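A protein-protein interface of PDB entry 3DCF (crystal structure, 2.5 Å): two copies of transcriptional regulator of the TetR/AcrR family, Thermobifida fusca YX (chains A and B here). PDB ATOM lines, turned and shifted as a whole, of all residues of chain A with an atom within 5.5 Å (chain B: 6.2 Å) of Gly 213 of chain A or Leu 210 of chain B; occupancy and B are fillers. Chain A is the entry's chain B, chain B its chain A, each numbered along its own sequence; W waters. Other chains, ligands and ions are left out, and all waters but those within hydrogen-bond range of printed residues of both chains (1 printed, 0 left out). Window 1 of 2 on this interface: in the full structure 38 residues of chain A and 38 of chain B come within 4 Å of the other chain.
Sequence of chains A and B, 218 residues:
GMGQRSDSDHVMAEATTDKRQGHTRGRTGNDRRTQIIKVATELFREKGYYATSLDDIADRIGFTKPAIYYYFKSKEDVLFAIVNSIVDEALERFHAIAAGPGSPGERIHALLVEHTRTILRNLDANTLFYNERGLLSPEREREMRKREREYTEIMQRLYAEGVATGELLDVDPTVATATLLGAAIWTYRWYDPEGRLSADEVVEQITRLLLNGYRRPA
Printed residues of chain B that touch a printed residue of chain A: Leu 112, Tyr 159, Leu 169, Thr 179, Leu 180, Ala 183, Ile 206, Leu 209, Leu 210, Leu 211, Asn 212, Gly 213 and Tyr 214.
Among the printed residues, no Asp or Glu carboxylate lies within 4 Å of a Lys or Arg side-chain nitrogen of the other chain.
Water W1 lies within hydrogen-bond range of the backbone carbonyl oxygen (O) of Arg 215 of chain A (3.0 Å) and the backbone carbonyl oxygen (O) of Leu 211 of chain B (3.4 Å).
Ile 206 of chain B touches Thr 179 of chain A.
Thr 179 of chain B touches Leu 209 of chain A.
CA of Gly 213 of chain B touches O of Leu 210 of chain A, at 3.2 Å.
CA of Gly 213 of chain B touches O of Leu 211 of chain A (3.5 Å).
Gly 213 of chain A touches Leu 210 of chain B (CA to O, 3.2 Å).
O of Leu 211 of chain B touches CA of Gly 213 of chain A, at 3.5 Å.
Gly 213 of chain A touches Asn 212 of chain B (CA to C, 3.7 Å).
Gly 213 of chain B touches Gly 213 of chain A (N to CA, 3.3 Å).
Tyr 214 of chain A touches Leu 112 of chain B.
CD2 of Leu 180 of chain B touches CD2 of Tyr 214 of chain A, 3.7 Å away.
Thr 179 of chain A touches Leu 209 of chain B, and with the chains exchanged Leu 209 of chain A touches Thr 179 of chain B.
Leu 211 of chain A touches Gly 213 of chain B, and with the chains exchanged Gly 213 of chain A touches Leu 211 of chain B.
Leu 211 of chain A touches Tyr 214 of chain B, and with the chains exchanged Tyr 214 of chain A touches Leu 211 of chain B.
Asn 212 of chain A touches its own counterpart, Asn 212 of chain B.
8 positions are printed for both chains.
Of the 25 pairs that touch across the chains among the printed residues, 14 have their exchanged pair printed and touching as well.
O of Asn 212 of chain B sits close to O of Asn 212 of chain A, 3.0 Å away.
The backbone NH (N) of Tyr 214 of chain B is in hydrogen-bond range of the backbone carbonyl oxygen (O) of Leu 211 of chain A.
N of Tyr 214 of chain B sits at hydrogen-bond distance from O of Leu 210 of chain A (3.2 Å).
The side-chain amide nitrogen (ND2) of Asn 212 of chain B lies close to the guanidinium group (NH2) of Arg 215 of chain A.
N of Tyr 214 of chain A lies within hydrogen-bond range of O of Leu 211 of chain B (3.4 Å).
The backbone NH of Arg 215 of chain A sits at hydrogen-bond distance from the backbone carbonyl oxygen of Leu 211 of chain B.
N of Tyr 214 of chain A sits close to O of Leu 210 of chain B, at 3.2 Å.
The backbone NH (N) of Leu 169 of chain B lies within hydrogen-bond range of the backbone carbonyl oxygen (O) of Tyr 214 of chain A (2.7 Å).
Of the printed residues of chain B, Gly 213 of chain A touches Leu 169 (3.7 Å), Leu 210 (3.2 Å), Leu 211 (3.5 Å), Asn 212 (3.7 Å) and Gly 213 (3.3 Å).
Printed residues of chain B within 4 Å of Tyr 214 of chain A: Leu 112 (3.7 Å), Leu 169 (2.7 Å), Leu 180 (3.7 Å), Leu 210 (3.1 Å) and Leu 211 (3.4 Å).
Of the printed residues of chain B, Arg 215 of chain A touches Leu 211 (3.4 Å) and Asn 212 (3.3 Å).
Thr 207 of chain B touches none of the printed residues of chain A.
Printed residues of chain A within 4 Å of Leu 210 of chain B: Gly 213 and Tyr 214.
Of the printed residues of chain A, Leu 211 of chain B touches Gly 213, Tyr 214 and Arg 215.
Of the printed residues of chain A, Tyr 214 of chain B touches Leu 210 (3.2 Å) and Leu 211 (3.4 Å).
The nearest residue of chain A that does not touch Leu 210 of chain B is Thr 179 of chain A (4.2 Å).
The nearest printed residue of chain A that does not touch Leu 209 of chain B is Leu 210 of chain A (4.8 Å).
The backbone carbonyl oxygen of Arg 208 of chain B lies close to the side-chain amide oxygen of Asn 212 of chain B, at 3.1 Å.
OH of Tyr 159 of chain B is in hydrogen-bond range of O of Leu 169 of chain B, at 2.7 Å.
The backbone carbonyl oxygen (O) of Arg 208 of chain A lies close to the side-chain amide oxygen (OD1) of Asn 212 of chain A, 3.0 Å away.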
ATOM      1  N   THR A 179       3.738   4.579  13.106  1.00  0.00           N
ATOM      2  CA  THR A 179       4.192   4.087  14.418  1.00  0.00           C
ATOM      3  C   THR A 179       5.574   4.635  14.801  1.00  0.00           C
ATOM      4  O   THR A 179       5.777   5.011  15.958  1.00  0.00           O
ATOM      5  CB  THR A 179       4.195   2.535  14.461  1.00  0.00           C
ATOM      6  OG1 THR A 179       2.862   2.060  14.203  1.00  0.00           O
ATOM      7  CG2 THR A 179       4.715   1.985  15.826  1.00  0.00           C
ATOM      8  N   ARG A 208      17.534   4.218  19.045  1.00  0.00           N
ATOM      9  CA  ARG A 208      18.142   2.894  19.310  1.00  0.00           C
ATOM     10  C   ARG A 208      17.062   1.855  19.677  1.00  0.00           C
ATOM     11  O   ARG A 208      17.196   0.666  19.339  1.00  0.00           O
ATOM     12  CB  ARG A 208      19.210   2.989  20.406  1.00  0.00           C
ATOM     13  CG  ARG A 208      19.987   1.683  20.661  1.00  0.00           C
ATOM     14  CD  ARG A 208      21.384   1.941  21.261  1.00  0.00           C
ATOM     15  NE  ARG A 208      21.342   2.676  22.533  1.00  0.00           N
ATOM     16  CZ  ARG A 208      21.235   2.145  23.758  1.00  0.00           C
ATOM     17  NH1 ARG A 208      21.139   0.822  23.957  1.00  0.00           N
ATOM     18  NH2 ARG A 208      21.206   2.973  24.810  1.00  0.00           N
ATOM     19  N   LEU A 209      16.009   2.310  20.368  1.00  0.00           N
ATOM     20  CA  LEU A 209      14.886   1.445  20.744  1.00  0.00           C
ATOM     21  C   LEU A 209      14.109   0.985  19.494  1.00  0.00           C
ATOM     22  O   LEU A 209      13.927  -0.212  19.273  1.00  0.00           O
ATOM     23  CB  LEU A 209      13.967   2.155  21.758  1.00  0.00           C
ATOM     24  CG  LEU A 209      12.810   1.362  22.389  1.00  0.00           C
ATOM     25  CD1 LEU A 209      13.311   0.185  23.243  1.00  0.00           C
ATOM     26  CD2 LEU A 209      11.946   2.293  23.210  1.00  0.00           C
ATOM     27  N   LEU A 210      13.705   1.937  18.659  1.00  0.00           N
ATOM     28  CA  LEU A 210      12.931   1.643  17.443  1.00  0.00           C
ATOM     29  C   LEU A 210      13.711   0.772  16.432  1.00  0.00           C
ATOM     30  O   LEU A 210      13.128  -0.091  15.800  1.00  0.00           O
ATOM     31  CB  LEU A 210      12.439   2.948  16.791  1.00  0.00           C
ATOM     32  CG  LEU A 210      11.530   3.863  17.644  1.00  0.00           C
ATOM     33  CD1 LEU A 210      11.299   5.234  16.989  1.00  0.00           C
ATOM     34  CD2 LEU A 210      10.201   3.193  17.971  1.00  0.00           C
ATOM     35  N   LEU A 211      15.022   0.980  16.328  1.00  0.00           N
ATOM     36  CA  LEU A 211      15.909   0.239  15.397  1.00  0.00           C
ATOM     37  C   LEU A 211      16.109  -1.254  15.724  1.00  0.00           C
ATOM     38  O   LEU A 211      15.956  -2.112  14.853  1.00  0.00           O
ATOM     39  CB  LEU A 211      17.281   0.943  15.340  1.00  0.00           C
ATOM     40  CG  LEU A 211      18.466   0.379  14.540  1.00  0.00           C
ATOM     41  CD1 LEU A 211      18.089   0.028  13.113  1.00  0.00           C
ATOM     42  CD2 LEU A 211      19.616   1.409  14.574  1.00  0.00           C
ATOM     43  N   ASN A 212      16.462  -1.527  16.979  1.00  0.00           N
ATOM     44  CA  ASN A 212      16.749  -2.881  17.482  1.00  0.00           C
ATOM     45  C   ASN A 212      15.569  -3.609  18.106  1.00  0.00           C
ATOM     46  O   ASN A 212      15.605  -4.838  18.246  1.00  0.00           O
ATOM     47  CB  ASN A 212      17.831  -2.809  18.579  1.00  0.00           C
ATOM     48  CG  ASN A 212      19.106  -2.166  18.107  1.00  0.00           C
ATOM     49  OD1 ASN A 212      19.529  -1.147  18.650  1.00  0.00           O
ATOM     50  ND2 ASN A 212      19.710  -2.732  17.073  1.00  0.00           N
ATOM     51  N   GLY A 213      14.548  -2.855  18.508  1.00  0.00           N
ATOM     52  CA  GLY A 213      13.427  -3.387  19.264  1.00  0.00           C
ATOM     53  C   GLY A 213      13.811  -3.400  20.745  1.00  0.00           C
ATOM     54  O   GLY A 213      14.958  -3.094  21.098  1.00  0.00           O
ATOM     55  N   TYR A 214      12.849  -3.728  21.615  1.00  0.00           N
ATOM     56  CA  TYR A 214      13.102  -3.784  23.071  1.00  0.00           C
ATOM     57  C   TYR A 214      13.683  -5.119  23.570  1.00  0.00           C
ATOM     58  O   TYR A 214      14.332  -5.132  24.606  1.00  0.00           O
ATOM     59  CB  TYR A 214      11.881  -3.349  23.901  1.00  0.00           C
ATOM     60  CG  TYR A 214      10.613  -4.176  23.787  1.00  0.00           C
ATOM     61  CD1 TYR A 214      10.398  -5.298  24.607  1.00  0.00           C
ATOM     62  CD2 TYR A 214       9.590  -3.801  22.904  1.00  0.00           C
ATOM     63  CE1 TYR A 214       9.206  -6.052  24.520  1.00  0.00           C
ATOM     64  CE2 TYR A 214       8.391  -4.547  22.809  1.00  0.00           C
ATOM     65  CZ  TYR A 214       8.210  -5.670  23.620  1.00  0.00           C
ATOM     66  OH  TYR A 214       7.048  -6.394  23.532  1.00  0.00           O
ATOM     67  N   ARG A 215      13.452  -6.218  22.848  1.00  0.00           N
ATOM     68  CA  ARG A 215      14.012  -7.529  23.210  1.00  0.00           C
ATOM     69  C   ARG A 215      15.422  -7.659  22.611  1.00  0.00           C
ATOM     70  O   ARG A 215      15.588  -7.451  21.404  1.00  0.00           O
ATOM     71  CB  ARG A 215      13.098  -8.665  22.709  1.00  0.00           C
ATOM     72  CG  ARG A 215      13.544 -10.093  23.136  1.00  0.00           C
ATOM     73  CD  ARG A 215      12.590 -11.176  22.633  1.00  0.00           C
ATOM     74  NE  ARG A 215      12.551 -11.263  21.165  1.00  0.00           N
ATOM     75  CZ  ARG A 215      11.802 -12.117  20.452  1.00  0.00           C
ATOM     76  NH1 ARG A 215      10.986 -13.011  21.040  1.00  0.00           N
ATOM     77  NH2 ARG A 215      11.861 -12.078  19.120  1.00  0.00           N
ATOM     78  N   LEU B 112       1.357  -4.554  25.867  1.00  0.00           N
ATOM     79  CA  LEU B 112       1.265  -3.751  24.630  1.00  0.00           C
ATOM     80  C   LEU B 112       0.147  -4.198  23.675  1.00  0.00           C
ATOM     81  O   LEU B 112      -0.525  -3.352  23.065  1.00  0.00           O
ATOM     82  CB  LEU B 112       2.614  -3.722  23.895  1.00  0.00           C
ATOM     83  CG  LEU B 112       3.728  -2.932  24.602  1.00  0.00           C
ATOM     84  CD1 LEU B 112       5.103  -3.172  23.924  1.00  0.00           C
ATOM     85  CD2 LEU B 112       3.405  -1.420  24.673  1.00  0.00           C
ATOM     86  N   TYR B 159      10.047  -2.874  33.067  1.00  0.00           N
ATOM     87  CA  TYR B 159      11.129  -2.671  32.078  1.00  0.00           C
ATOM     88  C   TYR B 159      12.519  -2.719  32.768  1.00  0.00           C
ATOM     89  O   TYR B 159      13.474  -3.235  32.174  1.00  0.00           O
ATOM     90  CB  TYR B 159      10.940  -1.382  31.249  1.00  0.00           C
ATOM     91  CG  TYR B 159      11.799  -1.356  29.997  1.00  0.00           C
ATOM     92  CD1 TYR B 159      13.127  -0.893  30.031  1.00  0.00           C
ATOM     93  CD2 TYR B 159      11.299  -1.803  28.774  1.00  0.00           C
ATOM     94  CE1 TYR B 159      13.934  -0.882  28.875  1.00  0.00           C
ATOM     95  CE2 TYR B 159      12.100  -1.794  27.604  1.00  0.00           C
ATOM     96  CZ  TYR B 159      13.420  -1.333  27.666  1.00  0.00           C
ATOM     97  OH  TYR B 159      14.218  -1.319  26.533  1.00  0.00           O
ATOM     98  N   LEU B 169      16.485  -4.352  26.019  1.00  0.00           N
ATOM     99  CA  LEU B 169      17.450  -3.323  25.553  1.00  0.00           C
ATOM    100  C   LEU B 169      17.749  -2.335  26.672  1.00  0.00           C
ATOM    101  O   LEU B 169      16.818  -1.791  27.280  1.00  0.00           O
ATOM    102  CB  LEU B 169      16.921  -2.535  24.337  1.00  0.00           C
ATOM    103  CG  LEU B 169      17.896  -1.528  23.682  1.00  0.00           C
ATOM    104  CD1 LEU B 169      19.031  -2.257  22.974  1.00  0.00           C
ATOM    105  CD2 LEU B 169      17.186  -0.607  22.717  1.00  0.00           C
ATOM    106  N   THR B 179       7.709   5.782  25.076  1.00  0.00           N
ATOM    107  CA  THR B 179       7.868   5.553  23.632  1.00  0.00           C
ATOM    108  C   THR B 179       7.016   4.378  23.133  1.00  0.00           C
ATOM    109  O   THR B 179       6.363   4.489  22.081  1.00  0.00           O
ATOM    110  CB  THR B 179       9.364   5.334  23.250  1.00  0.00           C
ATOM    111  OG1 THR B 179      10.128   6.505  23.588  1.00  0.00           O
ATOM    112  CG2 THR B 179       9.524   5.023  21.741  1.00  0.00           C
ATOM    113  N   LEU B 180       7.033   3.269  23.877  1.00  0.00           N
ATOM    114  CA  LEU B 180       6.275   2.058  23.503  1.00  0.00           C
ATOM    115  C   LEU B 180       4.768   2.297  23.625  1.00  0.00           C
ATOM    116  O   LEU B 180       4.012   1.957  22.708  1.00  0.00           O
ATOM    117  CB  LEU B 180       6.696   0.839  24.347  1.00  0.00           C
ATOM    118  CG  LEU B 180       8.133   0.274  24.271  1.00  0.00           C
ATOM    119  CD1 LEU B 180       8.319  -0.810  25.385  1.00  0.00           C
ATOM    120  CD2 LEU B 180       8.490  -0.260  22.875  1.00  0.00           C
ATOM    121  N   LEU B 181       4.344   2.869  24.763  1.00  0.00           N
ATOM    122  CA  LEU B 181       2.932   3.238  24.987  1.00  0.00           C
ATOM    123  C   LEU B 181       2.527   4.338  24.006  1.00  0.00           C
ATOM    124  O   LEU B 181       1.453   4.263  23.431  1.00  0.00           O
ATOM    125  CB  LEU B 181       2.672   3.688  26.434  1.00  0.00           C
ATOM    126  CG  LEU B 181       2.766   2.644  27.562  1.00  0.00           C
ATOM    127  CD1 LEU B 181       2.613   3.325  28.907  1.00  0.00           C
ATOM    128  CD2 LEU B 181       1.722   1.501  27.401  1.00  0.00           C
ATOM    129  N   ALA B 183       3.696   4.922  20.997  1.00  0.00           N
ATOM    130  CA  ALA B 183       3.534   4.281  19.670  1.00  0.00           C
ATOM    131  C   ALA B 183       2.163   3.598  19.542  1.00  0.00           C
ATOM    132  O   ALA B 183       1.548   3.649  18.484  1.00  0.00           O
ATOM    133  CB  ALA B 183       4.667   3.264  19.393  1.00  0.00           C
ATOM    134  N   ALA B 184       1.705   2.965  20.627  1.00  0.00           N
ATOM    135  CA  ALA B 184       0.384   2.316  20.687  1.00  0.00           C
ATOM    136  C   ALA B 184      -0.761   3.340  20.668  1.00  0.00           C
ATOM    137  O   ALA B 184      -1.726   3.168  19.927  1.00  0.00           O
ATOM    138  CB  ALA B 184       0.273   1.437  21.936  1.00  0.00           C
ATOM    139  N   GLN B 205       1.092  -6.240  13.898  1.00  0.00           N
ATOM    140  CA  GLN B 205       2.226  -5.575  13.224  1.00  0.00           C
ATOM    141  C   GLN B 205       2.945  -4.522  14.098  1.00  0.00           C
ATOM    142  O   GLN B 205       4.183  -4.492  14.132  1.00  0.00           O
ATOM    143  CB  GLN B 205       1.794  -4.982  11.879  1.00  0.00           C
ATOM    144  CG  GLN B 205       1.477  -6.043  10.837  1.00  0.00           C
ATOM    145  CD  GLN B 205       1.074  -5.486   9.471  1.00  0.00           C
ATOM    146  OE1 GLN B 205       1.347  -4.334   9.124  1.00  0.00           O
ATOM    147  NE2 GLN B 205       0.430  -6.329   8.678  1.00  0.00           N
ATOM    148  N   ILE B 206       2.165  -3.690  14.807  1.00  0.00           N
ATOM    149  CA  ILE B 206       2.702  -2.688  15.749  1.00  0.00           C
ATOM    150  C   ILE B 206       3.521  -3.383  16.846  1.00  0.00           C
ATOM    151  O   ILE B 206       4.660  -2.998  17.086  1.00  0.00           O
ATOM    152  CB  ILE B 206       1.589  -1.802  16.388  1.00  0.00           C
ATOM    153  CG1 ILE B 206       1.050  -0.805  15.362  1.00  0.00           C
ATOM    154  CG2 ILE B 206       2.117  -1.011  17.604  1.00  0.00           C
ATOM    155  CD1 ILE B 206      -0.178  -0.023  15.836  1.00  0.00           C
ATOM    156  N   THR B 207       2.943  -4.405  17.482  1.00  0.00           N
ATOM    157  CA  THR B 207       3.640  -5.159  18.556  1.00  0.00           C
ATOM    158  C   THR B 207       4.867  -5.964  18.029  1.00  0.00           C
ATOM    159  O   THR B 207       5.856  -6.145  18.754  1.00  0.00           O
ATOM    160  CB  THR B 207       2.672  -6.053  19.387  1.00  0.00           C
ATOM    161  OG1 THR B 207       2.056  -7.027  18.539  1.00  0.00           O
ATOM    162  CG2 THR B 207       1.598  -5.200  20.076  1.00  0.00           C
ATOM    163  N   ARG B 208       4.805  -6.423  16.782  1.00  0.00           N
ATOM    164  CA  ARG B 208       5.947  -7.101  16.141  1.00  0.00           C
ATOM    165  C   ARG B 208       7.052  -6.092  15.763  1.00  0.00           C
ATOM    166  O   ARG B 208       8.243  -6.425  15.826  1.00  0.00           O
ATOM    167  CB  ARG B 208       5.495  -7.903  14.910  1.00  0.00           C
ATOM    168  CG  ARG B 208       6.600  -8.771  14.253  1.00  0.00           C
ATOM    169  CD  ARG B 208       6.001  -9.982  13.494  1.00  0.00           C
ATOM    170  NE  ARG B 208       5.060  -9.590  12.435  1.00  0.00           N
ATOM    171  CZ  ARG B 208       5.372  -9.277  11.168  1.00  0.00           C
ATOM    172  NH1 ARG B 208       6.637  -9.276  10.722  1.00  0.00           N
ATOM    173  NH2 ARG B 208       4.386  -8.933  10.328  1.00  0.00           N
ATOM    174  N   LEU B 209       6.659  -4.875  15.368  1.00  0.00           N
ATOM    175  CA  LEU B 209       7.605  -3.805  15.029  1.00  0.00           C
ATOM    176  C   LEU B 209       8.390  -3.360  16.262  1.00  0.00           C
ATOM    177  O   LEU B 209       9.622  -3.340  16.235  1.00  0.00           O
ATOM    178  CB  LEU B 209       6.878  -2.617  14.391  1.00  0.00           C
ATOM    179  CG  LEU B 209       7.710  -1.459  13.835  1.00  0.00           C
ATOM    180  CD1 LEU B 209       8.618  -1.910  12.696  1.00  0.00           C
ATOM    181  CD2 LEU B 209       6.795  -0.379  13.366  1.00  0.00           C
ATOM    182  N   LEU B 210       7.682  -3.051  17.350  1.00  0.00           N
ATOM    183  CA  LEU B 210       8.310  -2.586  18.612  1.00  0.00           C
ATOM    184  C   LEU B 210       9.230  -3.630  19.286  1.00  0.00           C
ATOM    185  O   LEU B 210      10.248  -3.265  19.872  1.00  0.00           O
ATOM    186  CB  LEU B 210       7.232  -2.102  19.607  1.00  0.00           C
ATOM    187  CG  LEU B 210       6.317  -0.935  19.148  1.00  0.00           C
ATOM    188  CD1 LEU B 210       5.126  -0.716  20.121  1.00  0.00           C
ATOM    189  CD2 LEU B 210       7.100   0.351  18.912  1.00  0.00           C
ATOM    190  N   LEU B 211       8.859  -4.909  19.181  1.00  0.00           N
ATOM    191  CA  LEU B 211       9.604  -6.060  19.771  1.00  0.00           C
ATOM    192  C   LEU B 211      10.954  -6.366  19.115  1.00  0.00           C
ATOM    193  O   LEU B 211      11.965  -6.505  19.807  1.00  0.00           O
ATOM    194  CB  LEU B 211       8.718  -7.328  19.728  1.00  0.00           C
ATOM    195  CG  LEU B 211       9.236  -8.727  20.132  1.00  0.00           C
ATOM    196  CD1 LEU B 211       9.903  -8.753  21.492  1.00  0.00           C
ATOM    197  CD2 LEU B 211       8.069  -9.726  20.080  1.00  0.00           C
ATOM    198  N   ASN B 212      10.936  -6.487  17.788  1.00  0.00           N
ATOM    199  CA  ASN B 212      12.116  -6.821  16.963  1.00  0.00           C
ATOM    200  C   ASN B 212      12.879  -5.632  16.404  1.00  0.00           C
ATOM    201  O   ASN B 212      14.018  -5.799  15.947  1.00  0.00           O
ATOM    202  CB  ASN B 212      11.680  -7.633  15.732  1.00  0.00           C
ATOM    203  CG  ASN B 212      10.932  -8.891  16.087  1.00  0.00           C
ATOM    204  OD1 ASN B 212       9.790  -9.089  15.670  1.00  0.00           O
ATOM    205  ND2 ASN B 212      11.563  -9.744  16.876  1.00  0.00           N
ATOM    206  N   GLY B 213      12.236  -4.461  16.379  1.00  0.00           N
ATOM    207  CA  GLY B 213      12.780  -3.271  15.731  1.00  0.00           C
ATOM    208  C   GLY B 213      12.494  -3.338  14.228  1.00  0.00           C
ATOM    209  O   GLY B 213      11.989  -4.356  13.728  1.00  0.00           O
ATOM    210  N   TYR B 214      12.804  -2.262  13.502  1.00  0.00           N
ATOM    211  CA  TYR B 214      12.557  -2.213  12.043  1.00  0.00           C
ATOM    212  C   TYR B 214      13.656  -2.828  11.165  1.00  0.00           C
ATOM    213  O   TYR B 214      13.361  -3.234  10.042  1.00  0.00           O
ATOM    214  CB  TYR B 214      12.168  -0.807  11.558  1.00  0.00           C
ATOM    215  CG  TYR B 214      13.171   0.308  11.720  1.00  0.00           C
ATOM    216  CD1 TYR B 214      14.123   0.572  10.733  1.00  0.00           C
ATOM    217  CD2 TYR B 214      13.126   1.159  12.834  1.00  0.00           C
ATOM    218  CE1 TYR B 214      15.043   1.637  10.874  1.00  0.00           C
ATOM    219  CE2 TYR B 214      14.036   2.224  12.980  1.00  0.00           C
ATOM    220  CZ  TYR B 214      14.982   2.453  11.997  1.00  0.00           C
ATOM    221  OH  TYR B 214      15.858   3.484  12.151  1.00  0.00           O
HETATM  222  O   HOH W   1      14.307  -8.785  19.003  1.00  0.00           O
